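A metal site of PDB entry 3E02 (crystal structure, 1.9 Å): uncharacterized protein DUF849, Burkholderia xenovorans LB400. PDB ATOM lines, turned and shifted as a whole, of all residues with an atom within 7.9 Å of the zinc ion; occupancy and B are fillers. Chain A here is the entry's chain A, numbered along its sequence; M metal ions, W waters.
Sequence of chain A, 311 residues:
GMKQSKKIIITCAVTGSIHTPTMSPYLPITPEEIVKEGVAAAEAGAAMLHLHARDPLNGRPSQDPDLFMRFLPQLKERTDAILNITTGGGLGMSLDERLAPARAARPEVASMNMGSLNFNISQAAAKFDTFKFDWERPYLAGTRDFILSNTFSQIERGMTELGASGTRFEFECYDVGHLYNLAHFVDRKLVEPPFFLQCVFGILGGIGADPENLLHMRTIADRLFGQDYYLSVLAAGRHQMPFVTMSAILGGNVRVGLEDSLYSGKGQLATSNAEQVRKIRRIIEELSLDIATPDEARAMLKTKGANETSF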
ATOM      1  N   ALA A  13      11.987  17.344  20.123  1.00  0.00           N
ATOM      2  CA  ALA A  13      10.839  17.577  21.009  1.00  0.00           C
ATOM      3  C   ALA A  13      10.550  16.224  21.669  1.00  0.00           C
ATOM      4  O   ALA A  13       9.940  15.331  21.093  1.00  0.00           O
ATOM      5  CB  ALA A  13       9.649  18.120  20.236  1.00  0.00           C
ATOM      6  N   VAL A  14      11.004  16.101  22.912  1.00  0.00           N
ATOM      7  CA  VAL A  14      11.083  14.823  23.645  1.00  0.00           C
ATOM      8  C   VAL A  14       9.778  14.080  23.957  1.00  0.00           C
ATOM      9  O   VAL A  14       9.723  12.863  23.842  1.00  0.00           O
ATOM     10  CB  VAL A  14      11.933  15.009  24.957  1.00  0.00           C
ATOM     11  CG1 VAL A  14      11.973  13.733  25.815  1.00  0.00           C
ATOM     12  CG2 VAL A  14      13.379  15.447  24.590  1.00  0.00           C
ATOM     13  N   THR A  15       8.741  14.811  24.381  1.00  0.00           N
ATOM     14  CA  THR A  15       7.475  14.184  24.793  1.00  0.00           C
ATOM     15  C   THR A  15       6.196  14.966  24.528  1.00  0.00           C
ATOM     16  O   THR A  15       5.180  14.353  24.181  1.00  0.00           O
ATOM     17  CB  THR A  15       7.564  13.706  26.263  1.00  0.00           C
ATOM     18  OG1 THR A  15       6.481  12.809  26.539  1.00  0.00           O
ATOM     19  CG2 THR A  15       7.584  14.892  27.256  1.00  0.00           C
ATOM     20  N   GLY A  16       6.229  16.291  24.692  1.00  0.00           N
ATOM     21  CA  GLY A  16       5.051  17.096  24.407  1.00  0.00           C
ATOM     22  C   GLY A  16       3.884  16.857  25.340  1.00  0.00           C
ATOM     23  O   GLY A  16       4.053  16.381  26.471  1.00  0.00           O
ATOM     24  N   SER A  17       2.704  17.185  24.833  1.00  0.00           N
ATOM     25  CA  SER A  17       1.445  17.036  25.548  1.00  0.00           C
ATOM     26  C   SER A  17       0.276  16.537  24.683  1.00  0.00           C
ATOM     27  O   SER A  17      -0.831  16.459  25.222  1.00  0.00           O
ATOM     28  CB  SER A  17       1.075  18.414  26.125  1.00  0.00           C
ATOM     29  OG  SER A  17       0.764  19.309  25.063  1.00  0.00           O
ATOM     30  N   ILE A  18       0.496  16.171  23.414  1.00  0.00           N
ATOM     31  CA  ILE A  18      -0.547  15.701  22.463  1.00  0.00           C
ATOM     32  C   ILE A  18      -0.729  14.184  22.520  1.00  0.00           C
ATOM     33  O   ILE A  18      -1.857  13.682  22.544  1.00  0.00           O
ATOM     34  CB  ILE A  18      -0.178  16.085  20.977  1.00  0.00           C
ATOM     35  CG1 ILE A  18      -0.040  17.603  20.822  1.00  0.00           C
ATOM     36  CG2 ILE A  18      -1.190  15.526  19.970  1.00  0.00           C
ATOM     37  CD1 ILE A  18      -1.145  18.431  21.495  1.00  0.00           C
ATOM     38  N   HIS A  50      13.489  20.392  23.012  1.00  0.00           N
ATOM     39  CA  HIS A  50      12.241  21.086  23.314  1.00  0.00           C
ATOM     40  C   HIS A  50      11.529  20.226  24.368  1.00  0.00           C
ATOM     41  O   HIS A  50      11.230  19.056  24.142  1.00  0.00           O
ATOM     42  CB  HIS A  50      11.420  21.308  22.053  1.00  0.00           C
ATOM     43  CG  HIS A  50      10.045  21.815  22.308  1.00  0.00           C
ATOM     44  ND1 HIS A  50       9.770  23.121  22.624  1.00  0.00           N
ATOM     45  CD2 HIS A  50       8.863  21.161  22.328  1.00  0.00           C
ATOM     46  CE1 HIS A  50       8.466  23.251  22.818  1.00  0.00           C
ATOM     47  NE2 HIS A  50       7.895  22.082  22.615  1.00  0.00           N
ATOM     48  N   LEU A  51      11.252  20.830  25.526  1.00  0.00           N
ATOM     49  CA  LEU A  51      10.807  20.106  26.711  1.00  0.00           C
ATOM     50  C   LEU A  51       9.468  20.488  27.315  1.00  0.00           C
ATOM     51  O   LEU A  51       9.181  21.662  27.491  1.00  0.00           O
ATOM     52  CB  LEU A  51      11.874  20.294  27.783  1.00  0.00           C
ATOM     53  CG  LEU A  51      13.299  19.831  27.438  1.00  0.00           C
ATOM     54  CD1 LEU A  51      14.303  20.349  28.477  1.00  0.00           C
ATOM     55  CD2 LEU A  51      13.375  18.322  27.296  1.00  0.00           C
ATOM     56  N   HIS A  52       8.676  19.441  27.631  1.00  0.00           N
ATOM     57  CA  HIS A  52       7.447  19.499  28.412  1.00  0.00           C
ATOM     58  C   HIS A  52       7.639  18.537  29.589  1.00  0.00           C
ATOM     59  O   HIS A  52       8.494  17.634  29.535  1.00  0.00           O
ATOM     60  CB  HIS A  52       6.239  18.962  27.643  1.00  0.00           C
ATOM     61  CG  HIS A  52       5.797  19.791  26.488  1.00  0.00           C
ATOM     62  ND1 HIS A  52       4.501  20.252  26.349  1.00  0.00           N
ATOM     63  CD2 HIS A  52       6.465  20.195  25.379  1.00  0.00           C
ATOM     64  CE1 HIS A  52       4.405  20.925  25.218  1.00  0.00           C
ATOM     65  NE2 HIS A  52       5.582  20.902  24.609  1.00  0.00           N
ATOM     66  N   ASN A  84      15.137  24.120  25.521  1.00  0.00           N
ATOM     67  CA  ASN A  84      14.019  24.931  25.054  1.00  0.00           C
ATOM     68  C   ASN A  84      12.789  24.500  25.881  1.00  0.00           C
ATOM     69  O   ASN A  84      12.400  23.321  25.845  1.00  0.00           O
ATOM     70  CB  ASN A  84      13.911  24.693  23.526  1.00  0.00           C
ATOM     71  CG  ASN A  84      12.654  25.226  22.878  1.00  0.00           C
ATOM     72  OD1 ASN A  84      11.691  25.621  23.518  1.00  0.00           O
ATOM     73  ND2 ASN A  84      12.665  25.207  21.548  1.00  0.00           N
ATOM     74  N   ILE A  85      12.222  25.465  26.616  1.00  0.00           N
ATOM     75  CA  ILE A  85      11.063  25.239  27.496  1.00  0.00           C
ATOM     76  C   ILE A  85       9.757  25.664  26.820  1.00  0.00           C
ATOM     77  O   ILE A  85       9.642  26.779  26.271  1.00  0.00           O
ATOM     78  CB  ILE A  85      11.204  26.007  28.856  1.00  0.00           C
ATOM     79  CG1 ILE A  85      12.547  25.728  29.539  1.00  0.00           C
ATOM     80  CG2 ILE A  85      10.033  25.653  29.806  1.00  0.00           C
ATOM     81  CD1 ILE A  85      12.847  24.250  29.792  1.00  0.00           C
ATOM     82  N   THR A  86       8.764  24.777  26.882  1.00  0.00           N
ATOM     83  CA  THR A  86       7.469  25.073  26.322  1.00  0.00           C
ATOM     84  C   THR A  86       6.732  26.149  27.145  1.00  0.00           C
ATOM     85  O   THR A  86       6.855  26.196  28.371  1.00  0.00           O
ATOM     86  CB  THR A  86       6.543  23.818  26.244  1.00  0.00           C
ATOM     87  OG1 THR A  86       5.317  24.183  25.600  1.00  0.00           O
ATOM     88  CG2 THR A  86       6.241  23.252  27.631  1.00  0.00           C
ATOM     89  N   THR A  87       6.066  27.045  26.433  1.00  0.00           N
ATOM     90  CA  THR A  87       5.119  27.975  27.031  1.00  0.00           C
ATOM     91  C   THR A  87       3.711  27.609  26.498  1.00  0.00           C
ATOM     92  O   THR A  87       2.793  28.384  26.698  1.00  0.00           O
ATOM     93  CB  THR A  87       5.433  29.446  26.753  1.00  0.00           C
ATOM     94  OG1 THR A  87       5.258  29.713  25.368  1.00  0.00           O
ATOM     95  CG2 THR A  87       6.861  29.793  27.186  1.00  0.00           C
ATOM     96  N   GLY A  88       3.589  26.473  25.809  1.00  0.00           N
ATOM     97  CA  GLY A  88       2.324  25.922  25.303  1.00  0.00           C
ATOM     98  C   GLY A  88       1.798  24.980  26.375  1.00  0.00           C
ATOM     99  O   GLY A  88       0.670  25.106  26.821  1.00  0.00           O
ATOM    100  N   GLY A  89       2.658  24.055  26.804  1.00  0.00           N
ATOM    101  CA  GLY A  89       2.319  23.098  27.845  1.00  0.00           C
ATOM    102  C   GLY A  89       1.204  22.163  27.440  1.00  0.00           C
ATOM    103  O   GLY A  89       1.108  21.744  26.266  1.00  0.00           O
ATOM    104  N   SER A 111       9.525  28.272  23.733  1.00  0.00           N
ATOM    105  CA  SER A 111       8.605  28.254  22.587  1.00  0.00           C
ATOM    106  C   SER A 111       7.644  29.436  22.747  1.00  0.00           C
ATOM    107  O   SER A 111       7.404  29.894  23.867  1.00  0.00           O
ATOM    108  CB  SER A 111       7.866  26.912  22.449  1.00  0.00           C
ATOM    109  OG  SER A 111       7.021  26.672  23.538  1.00  0.00           O
ATOM    110  N   ASN A 113       3.994  30.474  20.879  1.00  0.00           N
ATOM    111  CA  ASN A 113       2.937  30.169  19.910  1.00  0.00           C
ATOM    112  C   ASN A 113       2.393  31.497  19.360  1.00  0.00           C
ATOM    113  O   ASN A 113       1.992  32.362  20.138  1.00  0.00           O
ATOM    114  CB  ASN A 113       1.896  29.311  20.571  1.00  0.00           C
ATOM    115  CG  ASN A 113       2.474  27.961  20.994  1.00  0.00           C
ATOM    116  OD1 ASN A 113       2.867  27.177  20.150  1.00  0.00           O
ATOM    117  ND2 ASN A 113       2.577  27.724  22.309  1.00  0.00           N
ATOM    118  N   GLU A 170      11.465  30.429  20.072  1.00  0.00           N
ATOM    119  CA  GLU A 170      11.193  29.501  18.972  1.00  0.00           C
ATOM    120  C   GLU A 170       9.742  29.913  18.640  1.00  0.00           C
ATOM    121  O   GLU A 170       8.823  29.548  19.368  1.00  0.00           O
ATOM    122  CB  GLU A 170      11.282  28.032  19.435  1.00  0.00           C
ATOM    123  CG  GLU A 170      10.964  26.916  18.382  1.00  0.00           C
ATOM    124  CD  GLU A 170      10.639  25.525  18.994  1.00  0.00           C
ATOM    125  OE1 GLU A 170      10.439  25.403  20.221  1.00  0.00           O
ATOM    126  OE2 GLU A 170      10.528  24.527  18.245  1.00  0.00           O
ATOM    127  N   GLU A 172       6.438  29.525  17.110  1.00  0.00           N
ATOM    128  CA  GLU A 172       5.645  28.417  16.529  1.00  0.00           C
ATOM    129  C   GLU A 172       4.537  29.014  15.680  1.00  0.00           C
ATOM    130  O   GLU A 172       3.647  29.669  16.203  1.00  0.00           O
ATOM    131  CB  GLU A 172       5.001  27.505  17.575  1.00  0.00           C
ATOM    132  CG  GLU A 172       5.820  27.161  18.777  1.00  0.00           C
ATOM    133  CD  GLU A 172       7.153  26.557  18.465  1.00  0.00           C
ATOM    134  OE1 GLU A 172       7.328  25.924  17.416  1.00  0.00           O
ATOM    135  OE2 GLU A 172       8.028  26.698  19.324  1.00  0.00           O
ATOM    136  N   TYR A 174       1.629  28.005  13.119  1.00  0.00           N
ATOM    137  CA  TYR A 174       0.736  26.929  12.664  1.00  0.00           C
ATOM    138  C   TYR A 174      -0.053  27.268  11.400  1.00  0.00           C
ATOM    139  O   TYR A 174      -0.803  26.433  10.908  1.00  0.00           O
ATOM    140  CB  TYR A 174      -0.291  26.579  13.751  1.00  0.00           C
ATOM    141  CG  TYR A 174       0.296  26.052  15.021  1.00  0.00           C
ATOM    142  CD1 TYR A 174       0.857  26.921  15.954  1.00  0.00           C
ATOM    143  CD2 TYR A 174       0.275  24.686  15.311  1.00  0.00           C
ATOM    144  CE1 TYR A 174       1.415  26.453  17.138  1.00  0.00           C
ATOM    145  CE2 TYR A 174       0.826  24.197  16.516  1.00  0.00           C
ATOM    146  CZ  TYR A 174       1.388  25.099  17.425  1.00  0.00           C
ATOM    147  OH  TYR A 174       1.931  24.688  18.609  1.00  0.00           O
ATOM    148  N   LEU A 234       8.387  21.297  11.673  1.00  0.00           N
ATOM    149  CA  LEU A 234       7.929  20.063  12.310  1.00  0.00           C
ATOM    150  C   LEU A 234       6.648  19.663  11.574  1.00  0.00           C
ATOM    151  O   LEU A 234       5.910  20.533  11.074  1.00  0.00           O
ATOM    152  CB  LEU A 234       7.661  20.226  13.805  1.00  0.00           C
ATOM    153  CG  LEU A 234       6.310  20.766  14.314  1.00  0.00           C
ATOM    154  CD1 LEU A 234       5.221  19.671  14.345  1.00  0.00           C
ATOM    155  CD2 LEU A 234       6.450  21.387  15.684  1.00  0.00           C
ATOM    156  N   ARG A 255      12.997  19.730  13.132  1.00  0.00           N
ATOM    157  CA  ARG A 255      12.514  19.292  14.434  1.00  0.00           C
ATOM    158  C   ARG A 255      11.909  17.897  14.298  1.00  0.00           C
ATOM    159  O   ARG A 255      11.039  17.700  13.456  1.00  0.00           O
ATOM    160  CB  ARG A 255      11.490  20.260  15.003  1.00  0.00           C
ATOM    161  CG  ARG A 255      10.705  19.679  16.168  1.00  0.00           C
ATOM    162  CD  ARG A 255      10.010  20.753  16.978  1.00  0.00           C
ATOM    163  NE  ARG A 255       8.838  20.190  17.642  1.00  0.00           N
ATOM    164  CZ  ARG A 255       8.061  20.844  18.498  1.00  0.00           C
ATOM    165  NH1 ARG A 255       8.358  22.071  18.932  1.00  0.00           N
ATOM    166  NH2 ARG A 255       6.989  20.222  18.971  1.00  0.00           N
ATOM    167  N   GLU A 259       7.261  13.855  20.704  1.00  0.00           N
ATOM    168  CA  GLU A 259       6.194  14.854  20.826  1.00  0.00           C
ATOM    169  C   GLU A 259       5.331  14.963  19.565  1.00  0.00           C
ATOM    170  O   GLU A 259       4.119  15.146  19.665  1.00  0.00           O
ATOM    171  CB  GLU A 259       6.791  16.216  21.139  1.00  0.00           C
ATOM    172  CG  GLU A 259       5.808  17.389  20.989  1.00  0.00           C
ATOM    173  CD  GLU A 259       6.172  18.632  21.742  1.00  0.00           C
ATOM    174  OE1 GLU A 259       7.138  18.635  22.511  1.00  0.00           O
ATOM    175  OE2 GLU A 259       5.394  19.581  21.586  1.00  0.00           O
ATOM    176  N   ASP A 260       5.981  14.861  18.406  1.00  0.00           N
ATOM    177  CA  ASP A 260       5.373  15.103  17.091  1.00  0.00           C
ATOM    178  C   ASP A 260       4.956  13.856  16.345  1.00  0.00           C
ATOM    179  O   ASP A 260       3.953  13.881  15.623  1.00  0.00           O
ATOM    180  CB  ASP A 260       6.364  15.891  16.200  1.00  0.00           C
ATOM    181  CG  ASP A 260       6.767  17.220  16.777  1.00  0.00           C
ATOM    182  OD1 ASP A 260       6.022  17.772  17.589  1.00  0.00           O
ATOM    183  OD2 ASP A 260       7.856  17.729  16.444  1.00  0.00           O
HETATM  184 ZN    ZN M   1       5.800  21.534  22.509  1.00  0.00          ZN
HETATM  185  O   HOH W   1       3.633  21.877  22.234  1.00  0.00           O
HETATM  186  O   HOH W   2       5.477  22.658  20.387  1.00  0.00           O
HETATM  187  O   HOH W   3       5.116  23.949  22.869  1.00  0.00           O
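ND1 of His 50 is in hydrogen-bond range of OE1 of Glu 170 (3.4 Å).
N of Val 14 sits at hydrogen-bond distance from O of His 50 (3.2 Å).
NE2 of His 52 sits close to OG1 of Thr 86, 3.4 Å away.
NH1 of Arg 255 lies within salt-bridge range of OE2 of Glu 170, 3.3 Å away.
N of Glu 259 is in hydrogen-bond range of O of Ala 13, 3.1 Å away.
A ring nitrogen (ND1) of His 50 is in hydrogen-bond range of the side-chain amide oxygen (OD1) of Asn 84, at 3.3 Å.
The backbone NH (N) of Gly 16 sits close to the side-chain carboxylate (OE1) of Glu 259 (3.3 Å).
OE1 of Glu 259 is in salt-bridge range of NH2 of Arg 255 (3.9 Å).
Residues that only touch the zinc ion: Arg 255 (3.96 Å).
Of the 24 residues printed, 4 come within 4 Å of the zinc ion.
The zinc ion is bound by a ring nitrogen (NE2) of His 50 (2.2 Å).
OE2 of Glu 259 binds the zinc ion, 2.2 Å away.
The zinc ion is bound by a ring nitrogen (NE2) of His 52 (2.2 Å).
Water W1 binds the zinc ion (2.2 Å).
Water W2 is bound to the zinc ion (2.4 Å).
The zinc ion is bound by water W3 (2.5 Å).
Water W3 bridges OG1 of Thr 86 (2.7 Å) and OG of Ser 111 (3.4 Å).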
